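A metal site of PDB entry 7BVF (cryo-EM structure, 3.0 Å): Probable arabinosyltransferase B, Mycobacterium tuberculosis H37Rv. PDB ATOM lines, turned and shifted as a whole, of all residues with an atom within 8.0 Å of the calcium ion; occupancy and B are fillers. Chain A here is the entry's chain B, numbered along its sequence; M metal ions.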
ATOM      1  N   GLY A 787      -8.325 -13.004  28.355  1.00  0.00           N
ATOM      2  CA  GLY A 787      -9.692 -12.992  27.893  1.00  0.00           C
ATOM      3  C   GLY A 787     -10.692 -12.459  28.908  1.00  0.00           C
ATOM      4  O   GLY A 787     -11.701 -11.877  28.515  1.00  0.00           O
ATOM      5  N   THR A 847     -16.238 -12.426  30.386  1.00  0.00           N
ATOM      6  CA  THR A 847     -15.728 -12.370  29.016  1.00  0.00           C
ATOM      7  C   THR A 847     -16.688 -11.666  28.081  1.00  0.00           C
ATOM      8  O   THR A 847     -16.927 -12.121  26.964  1.00  0.00           O
ATOM      9  CB  THR A 847     -15.436 -13.761  28.457  1.00  0.00           C
ATOM     10  OG1 THR A 847     -16.675 -14.408  28.149  1.00  0.00           O
ATOM     11  CG2 THR A 847     -14.698 -14.592  29.450  1.00  0.00           C
ATOM     12  N   TYR A 848     -17.254 -10.547  28.502  1.00  0.00           N
ATOM     13  CA  TYR A 848     -18.154  -9.765  27.657  1.00  0.00           C
ATOM     14  C   TYR A 848     -17.467  -8.478  27.246  1.00  0.00           C
ATOM     15  O   TYR A 848     -17.097  -7.665  28.102  1.00  0.00           O
ATOM     16  CB  TYR A 848     -19.467  -9.458  28.382  1.00  0.00           C
ATOM     17  CG  TYR A 848     -20.395  -8.570  27.592  1.00  0.00           C
ATOM     18  CD1 TYR A 848     -21.230  -9.108  26.629  1.00  0.00           C
ATOM     19  CD2 TYR A 848     -20.425  -7.202  27.795  1.00  0.00           C
ATOM     20  CE1 TYR A 848     -22.083  -8.307  25.903  1.00  0.00           C
ATOM     21  CE2 TYR A 848     -21.266  -6.400  27.075  1.00  0.00           C
ATOM     22  CZ  TYR A 848     -22.098  -6.956  26.128  1.00  0.00           C
ATOM     23  OH  TYR A 848     -22.939  -6.154  25.408  1.00  0.00           O
ATOM     24  N   THR A 849     -17.281  -8.294  25.945  1.00  0.00           N
ATOM     25  CA  THR A 849     -16.729  -7.077  25.385  1.00  0.00           C
ATOM     26  C   THR A 849     -17.558  -6.646  24.187  1.00  0.00           C
ATOM     27  O   THR A 849     -18.405  -7.388  23.688  1.00  0.00           O
ATOM     28  CB  THR A 849     -15.264  -7.261  24.952  1.00  0.00           C
ATOM     29  OG1 THR A 849     -15.167  -8.379  24.064  1.00  0.00           O
ATOM     30  CG2 THR A 849     -14.371  -7.496  26.150  1.00  0.00           C
ATOM     31  N   GLN A 853     -13.684  -9.597  19.496  1.00  0.00           N
ATOM     32  CA  GLN A 853     -13.817 -10.810  20.285  1.00  0.00           C
ATOM     33  C   GLN A 853     -12.546 -11.651  20.169  1.00  0.00           C
ATOM     34  O   GLN A 853     -11.700 -11.427  19.315  1.00  0.00           O
ATOM     35  CB  GLN A 853     -15.020 -11.629  19.816  1.00  0.00           C
ATOM     36  CG  GLN A 853     -16.285 -10.825  19.594  1.00  0.00           C
ATOM     37  CD  GLN A 853     -16.755 -10.118  20.843  1.00  0.00           C
ATOM     38  OE1 GLN A 853     -16.781  -8.898  20.899  1.00  0.00           O
ATOM     39  NE2 GLN A 853     -17.141 -10.896  21.850  1.00  0.00           N
ATOM     40  N   GLN A 854     -12.426 -12.644  21.053  1.00  0.00           N
ATOM     41  CA  GLN A 854     -11.277 -13.535  21.049  1.00  0.00           C
ATOM     42  C   GLN A 854     -11.644 -14.819  21.788  1.00  0.00           C
ATOM     43  O   GLN A 854     -12.767 -14.979  22.252  1.00  0.00           O
ATOM     44  CB  GLN A 854     -10.056 -12.850  21.667  1.00  0.00           C
ATOM     45  CG  GLN A 854     -10.311 -12.207  23.008  1.00  0.00           C
ATOM     46  CD  GLN A 854      -9.056 -11.657  23.637  1.00  0.00           C
ATOM     47  OE1 GLN A 854      -7.989 -12.268  23.557  1.00  0.00           O
ATOM     48  NE2 GLN A 854      -9.170 -10.493  24.271  1.00  0.00           N
ATOM     49  N   GLN A 855     -10.683 -15.728  21.879  1.00  0.00           N
ATOM     50  CA  GLN A 855     -10.832 -16.993  22.594  1.00  0.00           C
ATOM     51  C   GLN A 855     -10.309 -16.788  24.009  1.00  0.00           C
ATOM     52  O   GLN A 855      -9.116 -16.515  24.196  1.00  0.00           O
ATOM     53  CB  GLN A 855     -10.064 -18.111  21.896  1.00  0.00           C
ATOM     54  CG  GLN A 855     -10.753 -18.701  20.687  1.00  0.00           C
ATOM     55  CD  GLN A 855     -10.027 -19.907  20.157  1.00  0.00           C
ATOM     56  OE1 GLN A 855      -8.802 -19.979  20.217  1.00  0.00           O
ATOM     57  NE2 GLN A 855     -10.769 -20.863  19.629  1.00  0.00           N
ATOM     58  N   SER A 856     -11.180 -16.923  25.002  1.00  0.00           N
ATOM     59  CA  SER A 856     -10.761 -16.688  26.362  1.00  0.00           C
ATOM     60  C   SER A 856     -10.285 -17.978  27.026  1.00  0.00           C
ATOM     61  O   SER A 856     -10.272 -19.046  26.403  1.00  0.00           O
ATOM     62  CB  SER A 856     -11.893 -16.059  27.161  1.00  0.00           C
ATOM     63  OG  SER A 856     -12.397 -14.915  26.492  1.00  0.00           O
ATOM     64  N   GLN A 896     -20.592 -23.296  26.605  1.00  0.00           N
ATOM     65  CA  GLN A 896     -19.196 -23.160  26.982  1.00  0.00           C
ATOM     66  C   GLN A 896     -18.898 -24.068  28.179  1.00  0.00           C
ATOM     67  O   GLN A 896     -19.695 -24.927  28.538  1.00  0.00           O
ATOM     68  CB  GLN A 896     -18.862 -21.690  27.267  1.00  0.00           C
ATOM     69  CG  GLN A 896     -19.336 -20.721  26.189  1.00  0.00           C
ATOM     70  CD  GLN A 896     -18.847 -21.089  24.798  1.00  0.00           C
ATOM     71  OE1 GLN A 896     -17.755 -21.627  24.625  1.00  0.00           O
ATOM     72  NE2 GLN A 896     -19.672 -20.803  23.801  1.00  0.00           N
ATOM     73  N   GLU A 951     -13.639 -21.589  29.489  1.00  0.00           N
ATOM     74  CA  GLU A 951     -13.026 -21.508  28.162  1.00  0.00           C
ATOM     75  C   GLU A 951     -13.557 -20.372  27.292  1.00  0.00           C
ATOM     76  O   GLU A 951     -12.785 -19.481  26.948  1.00  0.00           O
ATOM     77  CB  GLU A 951     -13.184 -22.851  27.450  1.00  0.00           C
ATOM     78  CG  GLU A 951     -12.313 -23.930  28.029  1.00  0.00           C
ATOM     79  CD  GLU A 951     -10.852 -23.536  28.057  1.00  0.00           C
ATOM     80  OE1 GLU A 951     -10.365 -23.022  27.030  1.00  0.00           O
ATOM     81  OE2 GLU A 951     -10.192 -23.720  29.102  1.00  0.00           O
ATOM     82  N   ASP A 952     -14.854 -20.347  26.949  1.00  0.00           N
ATOM     83  CA  ASP A 952     -15.354 -19.363  25.979  1.00  0.00           C
ATOM     84  C   ASP A 952     -14.536 -19.300  24.685  1.00  0.00           C
ATOM     85  O   ASP A 952     -13.755 -18.364  24.483  1.00  0.00           O
ATOM     86  CB  ASP A 952     -15.441 -17.963  26.565  1.00  0.00           C
ATOM     87  CG  ASP A 952     -16.221 -17.023  25.675  1.00  0.00           C
ATOM     88  OD1 ASP A 952     -17.445 -17.193  25.565  1.00  0.00           O
ATOM     89  OD2 ASP A 952     -15.624 -16.122  25.056  1.00  0.00           O
ATOM     90  N   LEU A 953     -14.647 -20.334  23.862  1.00  0.00           N
ATOM     91  CA  LEU A 953     -13.993 -20.384  22.560  1.00  0.00           C
ATOM     92  C   LEU A 953     -14.843 -19.839  21.418  1.00  0.00           C
ATOM     93  O   LEU A 953     -14.452 -19.957  20.254  1.00  0.00           O
ATOM     94  CB  LEU A 953     -13.588 -21.831  22.234  1.00  0.00           C
ATOM     95  CG  LEU A 953     -12.714 -22.556  23.246  1.00  0.00           C
ATOM     96  CD1 LEU A 953     -12.668 -24.029  22.893  1.00  0.00           C
ATOM     97  CD2 LEU A 953     -11.319 -21.975  23.271  1.00  0.00           C
ATOM     98  N   SER A 954     -16.000 -19.242  21.705  1.00  0.00           N
ATOM     99  CA  SER A 954     -16.900 -18.744  20.685  1.00  0.00           C
ATOM    100  C   SER A 954     -16.748 -17.237  20.516  1.00  0.00           C
ATOM    101  O   SER A 954     -16.702 -16.494  21.505  1.00  0.00           O
ATOM    102  CB  SER A 954     -18.353 -19.076  21.007  1.00  0.00           C
ATOM    103  OG  SER A 954     -19.236 -18.207  20.332  1.00  0.00           O
ATOM    104  N   LEU A 955     -16.703 -16.776  19.271  1.00  0.00           N
ATOM    105  CA  LEU A 955     -16.470 -15.379  18.962  1.00  0.00           C
ATOM    106  C   LEU A 955     -17.748 -14.597  18.704  1.00  0.00           C
ATOM    107  O   LEU A 955     -17.684 -13.444  18.277  1.00  0.00           O
ATOM    108  CB  LEU A 955     -15.547 -15.247  17.747  1.00  0.00           C
ATOM    109  CG  LEU A 955     -14.224 -16.006  17.740  1.00  0.00           C
ATOM    110  CD1 LEU A 955     -13.331 -15.464  16.649  1.00  0.00           C
ATOM    111  CD2 LEU A 955     -13.537 -15.924  19.078  1.00  0.00           C
ATOM    112  N   THR A 956     -18.898 -15.194  18.955  1.00  0.00           N
ATOM    113  CA  THR A 956     -20.153 -14.456  18.830  1.00  0.00           C
ATOM    114  C   THR A 956     -20.254 -13.430  19.960  1.00  0.00           C
ATOM    115  O   THR A 956     -19.897 -13.721  21.099  1.00  0.00           O
ATOM    116  CB  THR A 956     -21.349 -15.414  18.888  1.00  0.00           C
ATOM    117  OG1 THR A 956     -21.293 -16.299  17.774  1.00  0.00           O
ATOM    118  CG2 THR A 956     -22.658 -14.658  18.846  1.00  0.00           C
ATOM    119  N   PRO A 957     -20.699 -12.206  19.662  1.00  0.00           N
ATOM    120  CA  PRO A 957     -20.802 -11.194  20.727  1.00  0.00           C
ATOM    121  C   PRO A 957     -21.768 -11.559  21.835  1.00  0.00           C
ATOM    122  O   PRO A 957     -21.685 -10.955  22.916  1.00  0.00           O
ATOM    123  CB  PRO A 957     -21.274  -9.941  19.960  1.00  0.00           C
ATOM    124  CG  PRO A 957     -20.785 -10.154  18.582  1.00  0.00           C
ATOM    125  CD  PRO A 957     -20.908 -11.622  18.328  1.00  0.00           C
ATOM    126  N   GLU A 958     -22.668 -12.507  21.625  1.00  0.00           N
ATOM    127  CA  GLU A 958     -23.636 -12.907  22.639  1.00  0.00           C
ATOM    128  C   GLU A 958     -23.358 -14.302  23.198  1.00  0.00           C
ATOM    129  O   GLU A 958     -24.273 -14.946  23.716  1.00  0.00           O
ATOM    130  CB  GLU A 958     -25.060 -12.829  22.080  1.00  0.00           C
ATOM    131  CG  GLU A 958     -25.306 -11.644  21.153  1.00  0.00           C
ATOM    132  CD  GLU A 958     -25.314 -10.291  21.853  1.00  0.00           C
ATOM    133  OE1 GLU A 958     -24.998 -10.220  23.065  1.00  0.00           O
ATOM    134  OE2 GLU A 958     -25.644  -9.295  21.196  1.00  0.00           O
ATOM    135  N   ASP A 959     -22.129 -14.780  23.088  1.00  0.00           N
ATOM    136  CA  ASP A 959     -21.682 -16.027  23.718  1.00  0.00           C
ATOM    137  C   ASP A 959     -20.564 -15.645  24.678  1.00  0.00           C
ATOM    138  O   ASP A 959     -19.395 -15.577  24.289  1.00  0.00           O
ATOM    139  CB  ASP A 959     -21.210 -17.035  22.679  1.00  0.00           C
ATOM    140  CG  ASP A 959     -22.333 -17.579  21.841  1.00  0.00           C
ATOM    141  OD1 ASP A 959     -22.089 -18.507  21.049  1.00  0.00           O
ATOM    142  OD2 ASP A 959     -23.477 -17.082  21.964  1.00  0.00           O
ATOM    143  N   TRP A 960     -20.923 -15.400  25.931  1.00  0.00           N
ATOM    144  CA  TRP A 960     -19.987 -14.929  26.944  1.00  0.00           C
ATOM    145  C   TRP A 960     -20.130 -15.795  28.195  1.00  0.00           C
ATOM    146  O   TRP A 960     -20.943 -16.705  28.254  1.00  0.00           O
ATOM    147  CB  TRP A 960     -20.210 -13.446  27.257  1.00  0.00           C
ATOM    148  CG  TRP A 960     -21.632 -13.117  27.556  1.00  0.00           C
ATOM    149  CD1 TRP A 960     -22.627 -12.876  26.657  1.00  0.00           C
ATOM    150  CD2 TRP A 960     -22.222 -12.974  28.846  1.00  0.00           C
ATOM    151  NE1 TRP A 960     -23.796 -12.611  27.313  1.00  0.00           N
ATOM    152  CE2 TRP A 960     -23.581 -12.663  28.661  1.00  0.00           C
ATOM    153  CE3 TRP A 960     -21.734 -13.089  30.156  1.00  0.00           C
ATOM    154  CZ2 TRP A 960     -24.441 -12.465  29.723  1.00  0.00           C
ATOM    155  CZ3 TRP A 960     -22.592 -12.889  31.196  1.00  0.00           C
ATOM    156  CH2 TRP A 960     -23.933 -12.576  30.985  1.00  0.00           C
ATOM    157  N   ILE A 961     -19.301 -15.482  29.192  1.00  0.00           N
ATOM    158  CA  ILE A 961     -19.147 -16.297  30.392  1.00  0.00           C
ATOM    159  C   ILE A 961     -18.823 -15.355  31.547  1.00  0.00           C
ATOM    160  O   ILE A 961     -18.200 -14.303  31.358  1.00  0.00           O
ATOM    161  CB  ILE A 961     -18.032 -17.361  30.193  1.00  0.00           C
ATOM    162  CG1 ILE A 961     -18.553 -18.559  29.404  1.00  0.00           C
ATOM    163  CG2 ILE A 961     -17.449 -17.844  31.501  1.00  0.00           C
ATOM    164  CD1 ILE A 961     -19.449 -19.451  30.185  1.00  0.00           C
HETATM  165 CA    CA M   1     -16.985 -14.877  23.403  1.00  0.00          CA
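The backbone carbonyl oxygen (O) of Asp 952 sits at hydrogen-bond distance from the backbone NH (N) of Ser 856 (3.0 Å). OG of Ser 954 lies within hydrogen-bond range of N of Thr 956 (3.3 Å).
Thr 956 touches the calcium ion. The nearest printed residue that does not touch the calcium ion is Gln 853 (4.3 Å).
The calcium ion is bound by the side-chain carboxylate of Asp 952 (2.5 Å), the backbone carbonyl oxygen of Ser 954 (2.5 Å) and the backbone carbonyl oxygen of Asp 959 (2.7 Å).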
